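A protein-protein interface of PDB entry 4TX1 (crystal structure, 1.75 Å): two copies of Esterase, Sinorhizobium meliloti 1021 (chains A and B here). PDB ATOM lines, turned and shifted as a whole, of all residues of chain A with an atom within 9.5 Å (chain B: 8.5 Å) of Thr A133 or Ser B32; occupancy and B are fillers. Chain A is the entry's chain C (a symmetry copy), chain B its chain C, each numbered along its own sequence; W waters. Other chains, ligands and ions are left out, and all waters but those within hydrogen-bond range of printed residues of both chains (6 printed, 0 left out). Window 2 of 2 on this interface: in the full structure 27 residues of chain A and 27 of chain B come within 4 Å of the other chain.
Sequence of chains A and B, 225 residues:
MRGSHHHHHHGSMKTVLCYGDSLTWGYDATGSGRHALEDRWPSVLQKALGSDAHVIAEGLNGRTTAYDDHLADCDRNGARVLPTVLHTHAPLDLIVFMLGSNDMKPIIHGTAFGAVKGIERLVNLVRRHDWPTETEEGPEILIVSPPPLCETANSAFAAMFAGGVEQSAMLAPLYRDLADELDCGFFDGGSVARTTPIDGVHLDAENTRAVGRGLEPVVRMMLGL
The indole nitrogen (NE1) of Trp B25 is in hydrogen-bond range of the backbone carbonyl oxygen (O) of Ala A90 (3.1 Å).
NH1 of Arg B34 is in hydrogen-bond range of O of His A89.
The backbone carbonyl oxygen (O) of Ala A90 lies within hydrogen-bond range of the guanidinium group (NH1) of Arg B34, at 2.8 Å.
O of Trp B25 sits at hydrogen-bond distance from NE of Arg B34 (2.9 Å).
The backbone carbonyl oxygen (O) of Tyr B27 sits at hydrogen-bond distance from a ring nitrogen (NE2) of His B35 (3.3 Å).
The backbone NH (N) of Asp B28 is in hydrogen-bond range of the backbone carbonyl oxygen (O) of Gly B33.
A ring nitrogen (NE2) of His A129 lies within hydrogen-bond range of a ring nitrogen (ND1) of His A87 (3.0 Å).
O of Thr A133 lies within hydrogen-bond range of OG1 of Thr A135 (2.6 Å).
His A87 touches Trp B25 (O to NE1, 3.6 Å).
CD of Pro A91 touches CD of Arg B34 (3.9 Å).
CZ2 of Trp B25 touches CG of Pro A132, at 3.8 Å.
Pro A132 touches Asn B61.
Thr A133 touches Trp B25.
Tyr B27 touches Thr A133.
CB of Thr A133 touches O of Ser B32 (3.6 Å).
Gly B33 touches Thr A133.
Thr A133 touches just these residues of chain B: Trp B25, Tyr B27, Ser B32 and Gly B33.
Of the printed residues of chain A, Ser B32 touches Thr A133 (3.6 Å).
Pro A132 touches just these residues of chain B: Trp B25 (3.8 Å) and Asn B61 (3.5 Å).
No residue of chain A comes within 4 Å of Gly B31.
Of the printed residues of chain B, Ala A90 touches Trp B25 and Arg B34.
Printed residues of chain A within 4 Å of Arg B34: His A89 (3.3 Å), Ala A90 (2.8 Å) and Pro A91 (3.9 Å).
Of the printed residues of chain A, Asn B61 touches Pro A132.
Printed residues of chain B within 4 Å of His A87: Trp B25 (3.6 Å).
The nearest residue of chain B that does not touch Thr A133 is Arg B34 (4.9 Å).
The nearest printed residue of chain B that does not touch His A89 is Trp B25 (4.6 Å).
Of the 15 printed residues of chain A, 6 touch a printed residue of chain B.
Hydrophobic or aromatic side chains of chain B within 4 Å of the printed part of chain A: Trp B25 and Tyr B27.
Among the printed residues, 11 pairs touch across the chains.
Among the printed residues, no Asp or Glu carboxylate lies within 4 Å of a Lys or Arg side-chain nitrogen of the other chain.
No position is printed for both chains.
Of the 11 pairs that touch across the chains among the printed residues, none has its exchanged pair printed and touching as well.
Water W3 lies within hydrogen-bond range of O of Pro A91, O of His A89 and NH1 of Arg B34.
Water W4 bridges ND1 of His A89 (2.8 Å) and NH2 of Arg B34 (2.8 Å).
Water W1 bridges O of Pro A132 (2.8 Å) and ND2 of Asn B61 (2.9 Å).
Water W2 lies within hydrogen-bond range of the backbone NH of Asn B61 (2.8 Å) and the backbone carbonyl oxygen of His A87 (2.9 Å).
Water W5 bridges O of Ser B32 and N of Glu A134.
Water W6 lies within hydrogen-bond range of the backbone carbonyl oxygen of Pro A132 (3.0 Å) and the side-chain hydroxyl of Tyr B27 (3.0 Å).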
ATOM      1  N   LEU A  86      13.226 -23.188   2.743  1.00  0.00           N
ATOM      2  CA  LEU A  86      13.513 -22.920   4.172  1.00  0.00           C
ATOM      3  C   LEU A  86      14.049 -21.564   4.327  1.00  0.00           C
ATOM      4  O   LEU A  86      13.651 -20.803   5.217  1.00  0.00           O
ATOM      5  CB  LEU A  86      14.500 -23.918   4.764  1.00  0.00           C
ATOM      6  CG  LEU A  86      14.067 -25.361   4.939  1.00  0.00           C
ATOM      7  CD1 LEU A  86      15.192 -26.286   5.430  1.00  0.00           C
ATOM      8  CD2 LEU A  86      12.794 -25.562   5.806  1.00  0.00           C
ATOM      9  N   HIS A  87      14.982 -21.195   3.460  1.00  0.00           N
ATOM     10  CA  HIS A  87      15.572 -19.865   3.567  1.00  0.00           C
ATOM     11  C   HIS A  87      14.639 -18.699   3.257  1.00  0.00           C
ATOM     12  O   HIS A  87      14.704 -17.654   3.889  1.00  0.00           O
ATOM     13  CB  HIS A  87      16.768 -19.788   2.562  1.00  0.00           C
ATOM     14  CG  HIS A  87      17.952 -19.011   3.066  1.00  0.00           C
ATOM     15  ND1 HIS A  87      18.803 -19.532   4.005  1.00  0.00           N
ATOM     16  CD2 HIS A  87      18.447 -17.797   2.729  1.00  0.00           C
ATOM     17  CE1 HIS A  87      19.749 -18.627   4.277  1.00  0.00           C
ATOM     18  NE2 HIS A  87      19.598 -17.600   3.486  1.00  0.00           N
ATOM     19  N   HIS A  89      11.446 -18.653   3.798  1.00  0.00           N
ATOM     20  CA  HIS A  89      10.369 -18.533   4.818  1.00  0.00           C
ATOM     21  C   HIS A  89      10.805 -18.516   6.263  1.00  0.00           C
ATOM     22  O   HIS A  89       9.969 -18.331   7.165  1.00  0.00           O
ATOM     23  CB  HIS A  89       9.301 -19.617   4.551  1.00  0.00           C
ATOM     24  CG  HIS A  89       8.639 -19.469   3.249  1.00  0.00           C
ATOM     25  ND1 HIS A  89       8.000 -18.318   2.850  1.00  0.00           N
ATOM     26  CD2 HIS A  89       8.578 -20.320   2.177  1.00  0.00           C
ATOM     27  CE1 HIS A  89       7.556 -18.460   1.622  1.00  0.00           C
ATOM     28  NE2 HIS A  89       7.895 -19.672   1.193  1.00  0.00           N
ATOM     29  N   ALA A  90      12.108 -18.628   6.502  1.00  0.00           N
ATOM     30  CA  ALA A  90      12.652 -18.548   7.900  1.00  0.00           C
ATOM     31  C   ALA A  90      12.308 -17.181   8.507  1.00  0.00           C
ATOM     32  O   ALA A  90      12.176 -16.246   7.813  1.00  0.00           O
ATOM     33  CB  ALA A  90      14.169 -18.672   7.869  1.00  0.00           C
ATOM     34  N   PRO A  91      12.257 -17.110   9.858  1.00  0.00           N
ATOM     35  CA  PRO A  91      12.390 -18.220  10.789  1.00  0.00           C
ATOM     36  C   PRO A  91      11.063 -19.028  10.918  1.00  0.00           C
ATOM     37  O   PRO A  91       9.941 -18.455  10.809  1.00  0.00           O
ATOM     38  CB  PRO A  91      12.679 -17.533  12.124  1.00  0.00           C
ATOM     39  CG  PRO A  91      12.086 -16.247  11.963  1.00  0.00           C
ATOM     40  CD  PRO A  91      12.150 -15.806  10.541  1.00  0.00           C
ATOM     41  N   LEU A  92      11.226 -20.312  11.127  1.00  0.00           N
ATOM     42  CA  LEU A  92      10.108 -21.284  11.109  1.00  0.00           C
ATOM     43  C   LEU A  92      10.029 -22.005  12.445  1.00  0.00           C
ATOM     44  O   LEU A  92      11.076 -22.435  13.015  1.00  0.00           O
ATOM     45  CB  LEU A  92      10.348 -22.331   9.978  1.00  0.00           C
ATOM     46  CG  LEU A  92      10.129 -21.715   8.601  1.00  0.00           C
ATOM     47  CD1 LEU A  92      10.738 -22.697   7.549  1.00  0.00           C
ATOM     48  CD2 LEU A  92       8.695 -21.443   8.299  1.00  0.00           C
ATOM     49  N   HIS A 129      20.137 -26.651   8.420  1.00  0.00           N
ATOM     50  CA  HIS A 129      20.005 -25.486   7.615  1.00  0.00           C
ATOM     51  C   HIS A 129      20.742 -24.312   8.186  1.00  0.00           C
ATOM     52  O   HIS A 129      20.636 -24.089   9.394  1.00  0.00           O
ATOM     53  CB  HIS A 129      18.543 -25.083   7.370  1.00  0.00           C
ATOM     54  CG  HIS A 129      18.420 -24.069   6.307  1.00  0.00           C
ATOM     55  ND1 HIS A 129      18.569 -24.405   4.975  1.00  0.00           N
ATOM     56  CD2 HIS A 129      18.350 -22.726   6.355  1.00  0.00           C
ATOM     57  CE1 HIS A 129      18.499 -23.308   4.268  1.00  0.00           C
ATOM     58  NE2 HIS A 129      18.380 -22.265   5.069  1.00  0.00           N
ATOM     59  N   ASP A 130      21.489 -23.586   7.347  1.00  0.00           N
ATOM     60  CA  ASP A 130      22.116 -22.267   7.761  1.00  0.00           C
ATOM     61  C   ASP A 130      21.197 -21.101   7.575  1.00  0.00           C
ATOM     62  O   ASP A 130      21.117 -20.510   6.502  1.00  0.00           O
ATOM     63  CB  ASP A 130      23.429 -22.043   6.977  1.00  0.00           C
ATOM     64  CG  ASP A 130      24.275 -20.878   7.580  1.00  0.00           C
ATOM     65  OD1 ASP A 130      24.207 -20.666   8.767  1.00  0.00           O
ATOM     66  OD2 ASP A 130      24.956 -20.211   6.818  1.00  0.00           O
ATOM     67  N   TRP A 131      20.410 -20.818   8.613  1.00  0.00           N
ATOM     68  CA  TRP A 131      19.340 -19.835   8.593  1.00  0.00           C
ATOM     69  C   TRP A 131      19.796 -18.450   8.191  1.00  0.00           C
ATOM     70  O   TRP A 131      20.982 -18.089   8.485  1.00  0.00           O
ATOM     71  CB  TRP A 131      18.670 -19.842   9.985  1.00  0.00           C
ATOM     72  CG  TRP A 131      18.135 -21.159  10.329  1.00  0.00           C
ATOM     73  CD1 TRP A 131      18.597 -22.008  11.204  1.00  0.00           C
ATOM     74  CD2 TRP A 131      16.985 -21.810   9.707  1.00  0.00           C
ATOM     75  NE1 TRP A 131      17.847 -23.200  11.203  1.00  0.00           N
ATOM     76  CE2 TRP A 131      16.815 -23.050  10.332  1.00  0.00           C
ATOM     77  CE3 TRP A 131      16.063 -21.415   8.780  1.00  0.00           C
ATOM     78  CZ2 TRP A 131      15.811 -23.956   9.930  1.00  0.00           C
ATOM     79  CZ3 TRP A 131      15.068 -22.315   8.417  1.00  0.00           C
ATOM     80  CH2 TRP A 131      14.958 -23.519   8.996  1.00  0.00           C
ATOM     81  N   PRO A 132      18.937 -17.629   7.569  1.00  0.00           N
ATOM     82  CA  PRO A 132      19.369 -16.310   7.031  1.00  0.00           C
ATOM     83  C   PRO A 132      19.805 -15.347   8.135  1.00  0.00           C
ATOM     84  O   PRO A 132      20.585 -14.459   7.856  1.00  0.00           O
ATOM     85  CB  PRO A 132      18.117 -15.706   6.415  1.00  0.00           C
ATOM     86  CG  PRO A 132      17.086 -16.754   6.448  1.00  0.00           C
ATOM     87  CD  PRO A 132      17.592 -17.996   7.104  1.00  0.00           C
ATOM     88  N   THR A 133      19.289 -15.572   9.340  1.00  0.00           N
ATOM     89  CA  THR A 133      19.621 -14.754  10.525  1.00  0.00           C
ATOM     90  C   THR A 133      19.789 -15.638  11.730  1.00  0.00           C
ATOM     91  O   THR A 133      19.440 -16.827  11.730  1.00  0.00           O
ATOM     92  CB  THR A 133      18.607 -13.654  10.823  1.00  0.00           C
ATOM     93  OG1 THR A 133      17.342 -14.247  11.070  1.00  0.00           O
ATOM     94  CG2 THR A 133      18.550 -12.605   9.671  1.00  0.00           C
ATOM     95  N   GLU A 134      20.392 -15.077  12.786  1.00  0.00           N
ATOM     96  CA  GLU A 134      20.812 -15.875  13.917  1.00  0.00           C
ATOM     97  C   GLU A 134      19.647 -16.548  14.575  1.00  0.00           C
ATOM     98  O   GLU A 134      18.655 -15.932  14.901  1.00  0.00           O
ATOM     99  CB  GLU A 134      21.575 -15.020  14.956  1.00  0.00           C
ATOM    100  CG  GLU A 134      22.375 -15.847  15.968  1.00  0.00           C
ATOM    101  CD  GLU A 134      23.834 -16.018  15.552  1.00  0.00           C
ATOM    102  OE1 GLU A 134      24.729 -15.521  16.273  1.00  0.00           O
ATOM    103  OE2 GLU A 134      24.095 -16.635  14.500  1.00  0.00           O
ATOM    104  N   THR A 135      19.789 -17.861  14.728  1.00  0.00           N
ATOM    105  CA  THR A 135      18.683 -18.674  15.122  1.00  0.00           C
ATOM    106  C   THR A 135      19.158 -19.594  16.252  1.00  0.00           C
ATOM    107  O   THR A 135      20.130 -20.344  16.088  1.00  0.00           O
ATOM    108  CB  THR A 135      18.208 -19.480  13.890  1.00  0.00           C
ATOM    109  OG1 THR A 135      17.814 -18.547  12.865  1.00  0.00           O
ATOM    110  CG2 THR A 135      17.009 -20.389  14.266  1.00  0.00           C
ATOM    111  N   GLU A 136      18.472 -19.523  17.381  1.00  0.00           N
ATOM    112  CA  GLU A 136      18.868 -20.336  18.548  1.00  0.00           C
ATOM    113  C   GLU A 136      18.506 -21.823  18.360  1.00  0.00           C
ATOM    114  O   GLU A 136      19.344 -22.688  18.563  1.00  0.00           O
ATOM    115  CB  GLU A 136      18.211 -19.850  19.840  1.00  0.00           C
ATOM    116  CG  GLU A 136      17.596 -18.456  19.805  1.00  0.00           C
ATOM    117  CD  GLU A 136      17.528 -17.802  21.180  1.00  0.00           C
ATOM    118  OE1 GLU A 136      16.562 -17.047  21.443  1.00  0.00           O
ATOM    119  OE2 GLU A 136      18.453 -18.035  21.994  1.00  0.00           O
ATOM    120  N   GLU A 137      17.260 -22.085  17.956  1.00  0.00           N
ATOM    121  CA  GLU A 137      16.669 -23.444  17.999  1.00  0.00           C
ATOM    122  C   GLU A 137      16.132 -23.921  16.636  1.00  0.00           C
ATOM    123  O   GLU A 137      15.562 -23.136  15.904  1.00  0.00           O
ATOM    124  CB  GLU A 137      15.517 -23.525  19.036  1.00  0.00           C
ATOM    125  CG  GLU A 137      15.333 -22.307  19.924  1.00  0.00           C
ATOM    126  CD  GLU A 137      14.750 -21.108  19.175  1.00  0.00           C
ATOM    127  OE1 GLU A 137      13.661 -20.645  19.583  1.00  0.00           O
ATOM    128  OE2 GLU A 137      15.365 -20.626  18.183  1.00  0.00           O
ATOM    129  N   TRP B  25      11.744 -10.449   1.607  1.00  0.00           N
ATOM    130  CA  TRP B  25      11.804 -11.262   2.806  1.00  0.00           C
ATOM    131  C   TRP B  25      11.484 -10.375   4.030  1.00  0.00           C
ATOM    132  O   TRP B  25      10.709 -10.774   4.871  1.00  0.00           O
ATOM    133  CB  TRP B  25      13.178 -11.876   3.008  1.00  0.00           C
ATOM    134  CG  TRP B  25      13.341 -12.843   4.127  1.00  0.00           C
ATOM    135  CD1 TRP B  25      12.862 -14.110   4.244  1.00  0.00           C
ATOM    136  CD2 TRP B  25      14.073 -12.625   5.361  1.00  0.00           C
ATOM    137  NE1 TRP B  25      13.256 -14.713   5.388  1.00  0.00           N
ATOM    138  CE2 TRP B  25      13.976 -13.797   6.119  1.00  0.00           C
ATOM    139  CE3 TRP B  25      14.799 -11.535   5.884  1.00  0.00           C
ATOM    140  CZ2 TRP B  25      14.607 -13.977   7.345  1.00  0.00           C
ATOM    141  CZ3 TRP B  25      15.419 -11.712   7.103  1.00  0.00           C
ATOM    142  CH2 TRP B  25      15.336 -12.883   7.834  1.00  0.00           C
ATOM    143  N   GLY B  26      12.101  -9.205   4.001  1.00  0.00           N
ATOM    144  CA  GLY B  26      11.914  -8.128   5.046  1.00  0.00           C
ATOM    145  C   GLY B  26      13.092  -8.137   6.024  1.00  0.00           C
ATOM    146  O   GLY B  26      12.961  -8.502   7.245  1.00  0.00           O
ATOM    147  N   TYR B  27      14.272  -7.791   5.523  1.00  0.00           N
ATOM    148  CA  TYR B  27      15.481  -7.849   6.342  1.00  0.00           C
ATOM    149  C   TYR B  27      15.543  -6.641   7.282  1.00  0.00           C
ATOM    150  O   TYR B  27      15.518  -5.562   6.837  1.00  0.00           O
ATOM    151  CB  TYR B  27      16.759  -7.946   5.479  1.00  0.00           C
ATOM    152  CG  TYR B  27      17.970  -8.279   6.293  1.00  0.00           C
ATOM    153  CD1 TYR B  27      18.305  -9.550   6.516  1.00  0.00           C
ATOM    154  CD2 TYR B  27      18.746  -7.307   6.855  1.00  0.00           C
ATOM    155  CE1 TYR B  27      19.354  -9.889   7.298  1.00  0.00           C
ATOM    156  CE2 TYR B  27      19.814  -7.631   7.638  1.00  0.00           C
ATOM    157  CZ  TYR B  27      20.101  -8.936   7.863  1.00  0.00           C
ATOM    158  OH  TYR B  27      21.144  -9.332   8.627  1.00  0.00           O
ATOM    159  N   ASP B  28      15.600  -6.886   8.587  1.00  0.00           N
ATOM    160  CA  ASP B  28      15.743  -5.767   9.622  1.00  0.00           C
ATOM    161  C   ASP B  28      17.232  -5.588  10.011  1.00  0.00           C
ATOM    162  O   ASP B  28      17.770  -6.355  10.802  1.00  0.00           O
ATOM    163  CB  ASP B  28      14.892  -6.128  10.814  1.00  0.00           C
ATOM    164  CG  ASP B  28      15.235  -5.334  12.097  1.00  0.00           C
ATOM    165  OD1 ASP B  28      15.606  -4.167  11.905  1.00  0.00           O
ATOM    166  OD2 ASP B  28      15.143  -5.925  13.236  1.00  0.00           O
ATOM    167  N   ALA B  29      17.825  -4.610   9.409  1.00  0.00           N
ATOM    168  CA  ALA B  29      19.262  -4.331   9.546  1.00  0.00           C
ATOM    169  C   ALA B  29      19.547  -3.731  10.930  1.00  0.00           C
ATOM    170  O   ALA B  29      20.703  -3.741  11.375  1.00  0.00           O
ATOM    171  CB  ALA B  29      19.727  -3.399   8.515  1.00  0.00           C
ATOM    172  N   THR B  30      18.514  -3.169  11.551  1.00  0.00           N
ATOM    173  CA  THR B  30      18.724  -2.574  12.886  1.00  0.00           C
ATOM    174  C   THR B  30      18.957  -3.697  13.856  1.00  0.00           C
ATOM    175  O   THR B  30      19.871  -3.625  14.712  1.00  0.00           O
ATOM    176  CB  THR B  30      17.447  -1.782  13.333  1.00  0.00           C
ATOM    177  OG1 THR B  30      17.349  -0.605  12.504  1.00  0.00           O
ATOM    178  CG2 THR B  30      17.572  -1.384  14.773  1.00  0.00           C
ATOM    179  N   GLY B  31      18.114  -4.743  13.745  1.00  0.00           N
ATOM    180  CA  GLY B  31      18.122  -5.898  14.647  1.00  0.00           C
ATOM    181  C   GLY B  31      18.797  -7.140  14.080  1.00  0.00           C
ATOM    182  O   GLY B  31      18.932  -8.099  14.799  1.00  0.00           O
ATOM    183  N   SER B  32      19.224  -7.112  12.813  1.00  0.00           N
ATOM    184  CA  SER B  32      19.808  -8.334  12.126  1.00  0.00           C
ATOM    185  C   SER B  32      18.799  -9.498  12.219  1.00  0.00           C
ATOM    186  O   SER B  32      19.093 -10.596  12.728  1.00  0.00           O
ATOM    187  CB  SER B  32      21.183  -8.706  12.708  1.00  0.00           C
ATOM    188  OG  SER B  32      22.149  -7.644  12.528  1.00  0.00           O
ATOM    189  N   GLY B  33      17.575  -9.213  11.841  1.00  0.00           N
ATOM    190  CA  GLY B  33      16.491 -10.190  12.020  1.00  0.00           C
ATOM    191  C   GLY B  33      15.517  -9.932  10.884  1.00  0.00           C
ATOM    192  O   GLY B  33      15.875  -9.292   9.891  1.00  0.00           O
ATOM    193  N   ARG B  34      14.274 -10.393  11.064  1.00  0.00           N
ATOM    194  CA  ARG B  34      13.236 -10.242  10.034  1.00  0.00           C
ATOM    195  C   ARG B  34      12.163  -9.253  10.514  1.00  0.00           C
ATOM    196  O   ARG B  34      11.767  -9.376  11.673  1.00  0.00           O
ATOM    197  CB  ARG B  34      12.596 -11.592   9.686  1.00  0.00           C
ATOM    198  CG  ARG B  34      11.775 -11.555   8.440  1.00  0.00           C
ATOM    199  CD  ARG B  34      11.240 -12.967   8.079  1.00  0.00           C
ATOM    200  NE  ARG B  34      10.635 -12.907   6.766  1.00  0.00           N
ATOM    201  CZ  ARG B  34       9.928 -13.907   6.216  1.00  0.00           C
ATOM    202  NH1 ARG B  34       9.831 -15.065   6.847  1.00  0.00           N
ATOM    203  NH2 ARG B  34       9.395 -13.700   5.047  1.00  0.00           N
ATOM    204  N   HIS B  35      11.747  -8.326   9.664  1.00  0.00           N
ATOM    205  CA  HIS B  35      10.607  -7.469   9.981  1.00  0.00           C
ATOM    206  C   HIS B  35       9.408  -8.324  10.347  1.00  0.00           C
ATOM    207  O   HIS B  35       9.199  -9.425   9.815  1.00  0.00           O
ATOM    208  CB  HIS B  35      10.238  -6.595   8.808  1.00  0.00           C
ATOM    209  CG  HIS B  35      11.245  -5.576   8.414  1.00  0.00           C
ATOM    210  ND1 HIS B  35      11.876  -4.750   9.345  1.00  0.00           N
ATOM    211  CD2 HIS B  35      11.661  -5.169   7.200  1.00  0.00           C
ATOM    212  CE1 HIS B  35      12.663  -3.916   8.693  1.00  0.00           C
ATOM    213  NE2 HIS B  35      12.553  -4.137   7.381  1.00  0.00           N
ATOM    214  N   ASN B  61      16.794 -13.919   0.576  1.00  0.00           N
ATOM    215  CA  ASN B  61      17.964 -13.021   0.837  1.00  0.00           C
ATOM    216  C   ASN B  61      19.087 -13.419  -0.171  1.00  0.00           C
ATOM    217  O   ASN B  61      19.471 -14.562  -0.269  1.00  0.00           O
ATOM    218  CB  ASN B  61      18.431 -13.200   2.267  1.00  0.00           C
ATOM    219  CG  ASN B  61      17.434 -12.649   3.277  1.00  0.00           C
ATOM    220  OD1 ASN B  61      16.322 -12.250   2.924  1.00  0.00           O
ATOM    221  ND2 ASN B  61      17.802 -12.779   4.573  1.00  0.00           N
ATOM    222  N   PHE B 157      29.849  -4.305   3.632  1.00  0.00           N
ATOM    223  CA  PHE B 157      28.880  -3.963   2.625  1.00  0.00           C
ATOM    224  C   PHE B 157      29.376  -3.043   1.563  1.00  0.00           C
ATOM    225  O   PHE B 157      28.961  -3.113   0.414  1.00  0.00           O
ATOM    226  CB  PHE B 157      27.571  -3.451   3.284  1.00  0.00           C
ATOM    227  CG  PHE B 157      26.657  -4.565   3.765  1.00  0.00           C
ATOM    228  CD1 PHE B 157      26.830  -5.212   4.976  1.00  0.00           C
ATOM    229  CD2 PHE B 157      25.608  -4.961   2.923  1.00  0.00           C
ATOM    230  CE1 PHE B 157      25.979  -6.255   5.347  1.00  0.00           C
ATOM    231  CE2 PHE B 157      24.746  -5.972   3.309  1.00  0.00           C
ATOM    232  CZ  PHE B 157      24.947  -6.643   4.507  1.00  0.00           C
ATOM    233  N   ILE B 198      22.874   1.743   7.376  1.00  0.00           N
ATOM    234  CA  ILE B 198      23.370   0.700   8.211  1.00  0.00           C
ATOM    235  C   ILE B 198      24.242  -0.167   7.277  1.00  0.00           C
ATOM    236  O   ILE B 198      25.307  -0.680   7.712  1.00  0.00           O
ATOM    237  CB  ILE B 198      22.291  -0.104   8.973  1.00  0.00           C
ATOM    238  CG1 ILE B 198      21.491   0.812   9.966  1.00  0.00           C
ATOM    239  CG2 ILE B 198      22.863  -1.369   9.662  1.00  0.00           C
ATOM    240  CD1 ILE B 198      20.231   0.163  10.588  1.00  0.00           C
ATOM    241  N   ASP B 199      23.688  -0.491   6.115  1.00  0.00           N
ATOM    242  CA  ASP B 199      24.390  -1.394   5.147  1.00  0.00           C
ATOM    243  C   ASP B 199      24.280  -1.004   3.723  1.00  0.00           C
ATOM    244  O   ASP B 199      24.872  -1.653   2.831  1.00  0.00           O
ATOM    245  CB  ASP B 199      23.966  -2.867   5.360  1.00  0.00           C
ATOM    246  CG  ASP B 199      22.472  -3.080   5.234  1.00  0.00           C
ATOM    247  OD1 ASP B 199      21.906  -2.365   4.412  1.00  0.00           O
ATOM    248  OD2 ASP B 199      21.988  -4.054   5.945  1.00  0.00           O
ATOM    249  N   HIS B 202      19.349  -2.376   2.586  1.00  0.00           N
ATOM    250  CA  HIS B 202      18.132  -2.818   3.245  1.00  0.00           C
ATOM    251  C   HIS B 202      17.142  -1.630   3.480  1.00  0.00           C
ATOM    252  O   HIS B 202      17.505  -0.482   3.206  1.00  0.00           O
ATOM    253  CB  HIS B 202      18.459  -3.645   4.447  1.00  0.00           C
ATOM    254  CG  HIS B 202      19.084  -4.980   4.121  1.00  0.00           C
ATOM    255  ND1 HIS B 202      20.299  -5.379   4.641  1.00  0.00           N
ATOM    256  CD2 HIS B 202      18.637  -6.021   3.342  1.00  0.00           C
ATOM    257  CE1 HIS B 202      20.569  -6.620   4.206  1.00  0.00           C
ATOM    258  NE2 HIS B 202      19.595  -7.015   3.389  1.00  0.00           N
HETATM  259  O   HOH W   1      20.579 -13.440   5.255  1.00  0.00           O
HETATM  260  O   HOH W   2      15.669 -15.161   2.860  1.00  0.00           O
HETATM  261  O   HOH W   3       8.851 -16.792   9.146  1.00  0.00           O
HETATM  262  O   HOH W   4       7.870 -15.971   4.331  1.00  0.00           O
HETATM  263  O   HOH W   5      21.334 -12.340  12.672  1.00  0.00           O
HETATM  264  O   HOH W   6      21.975 -12.147   9.106  1.00  0.00           O
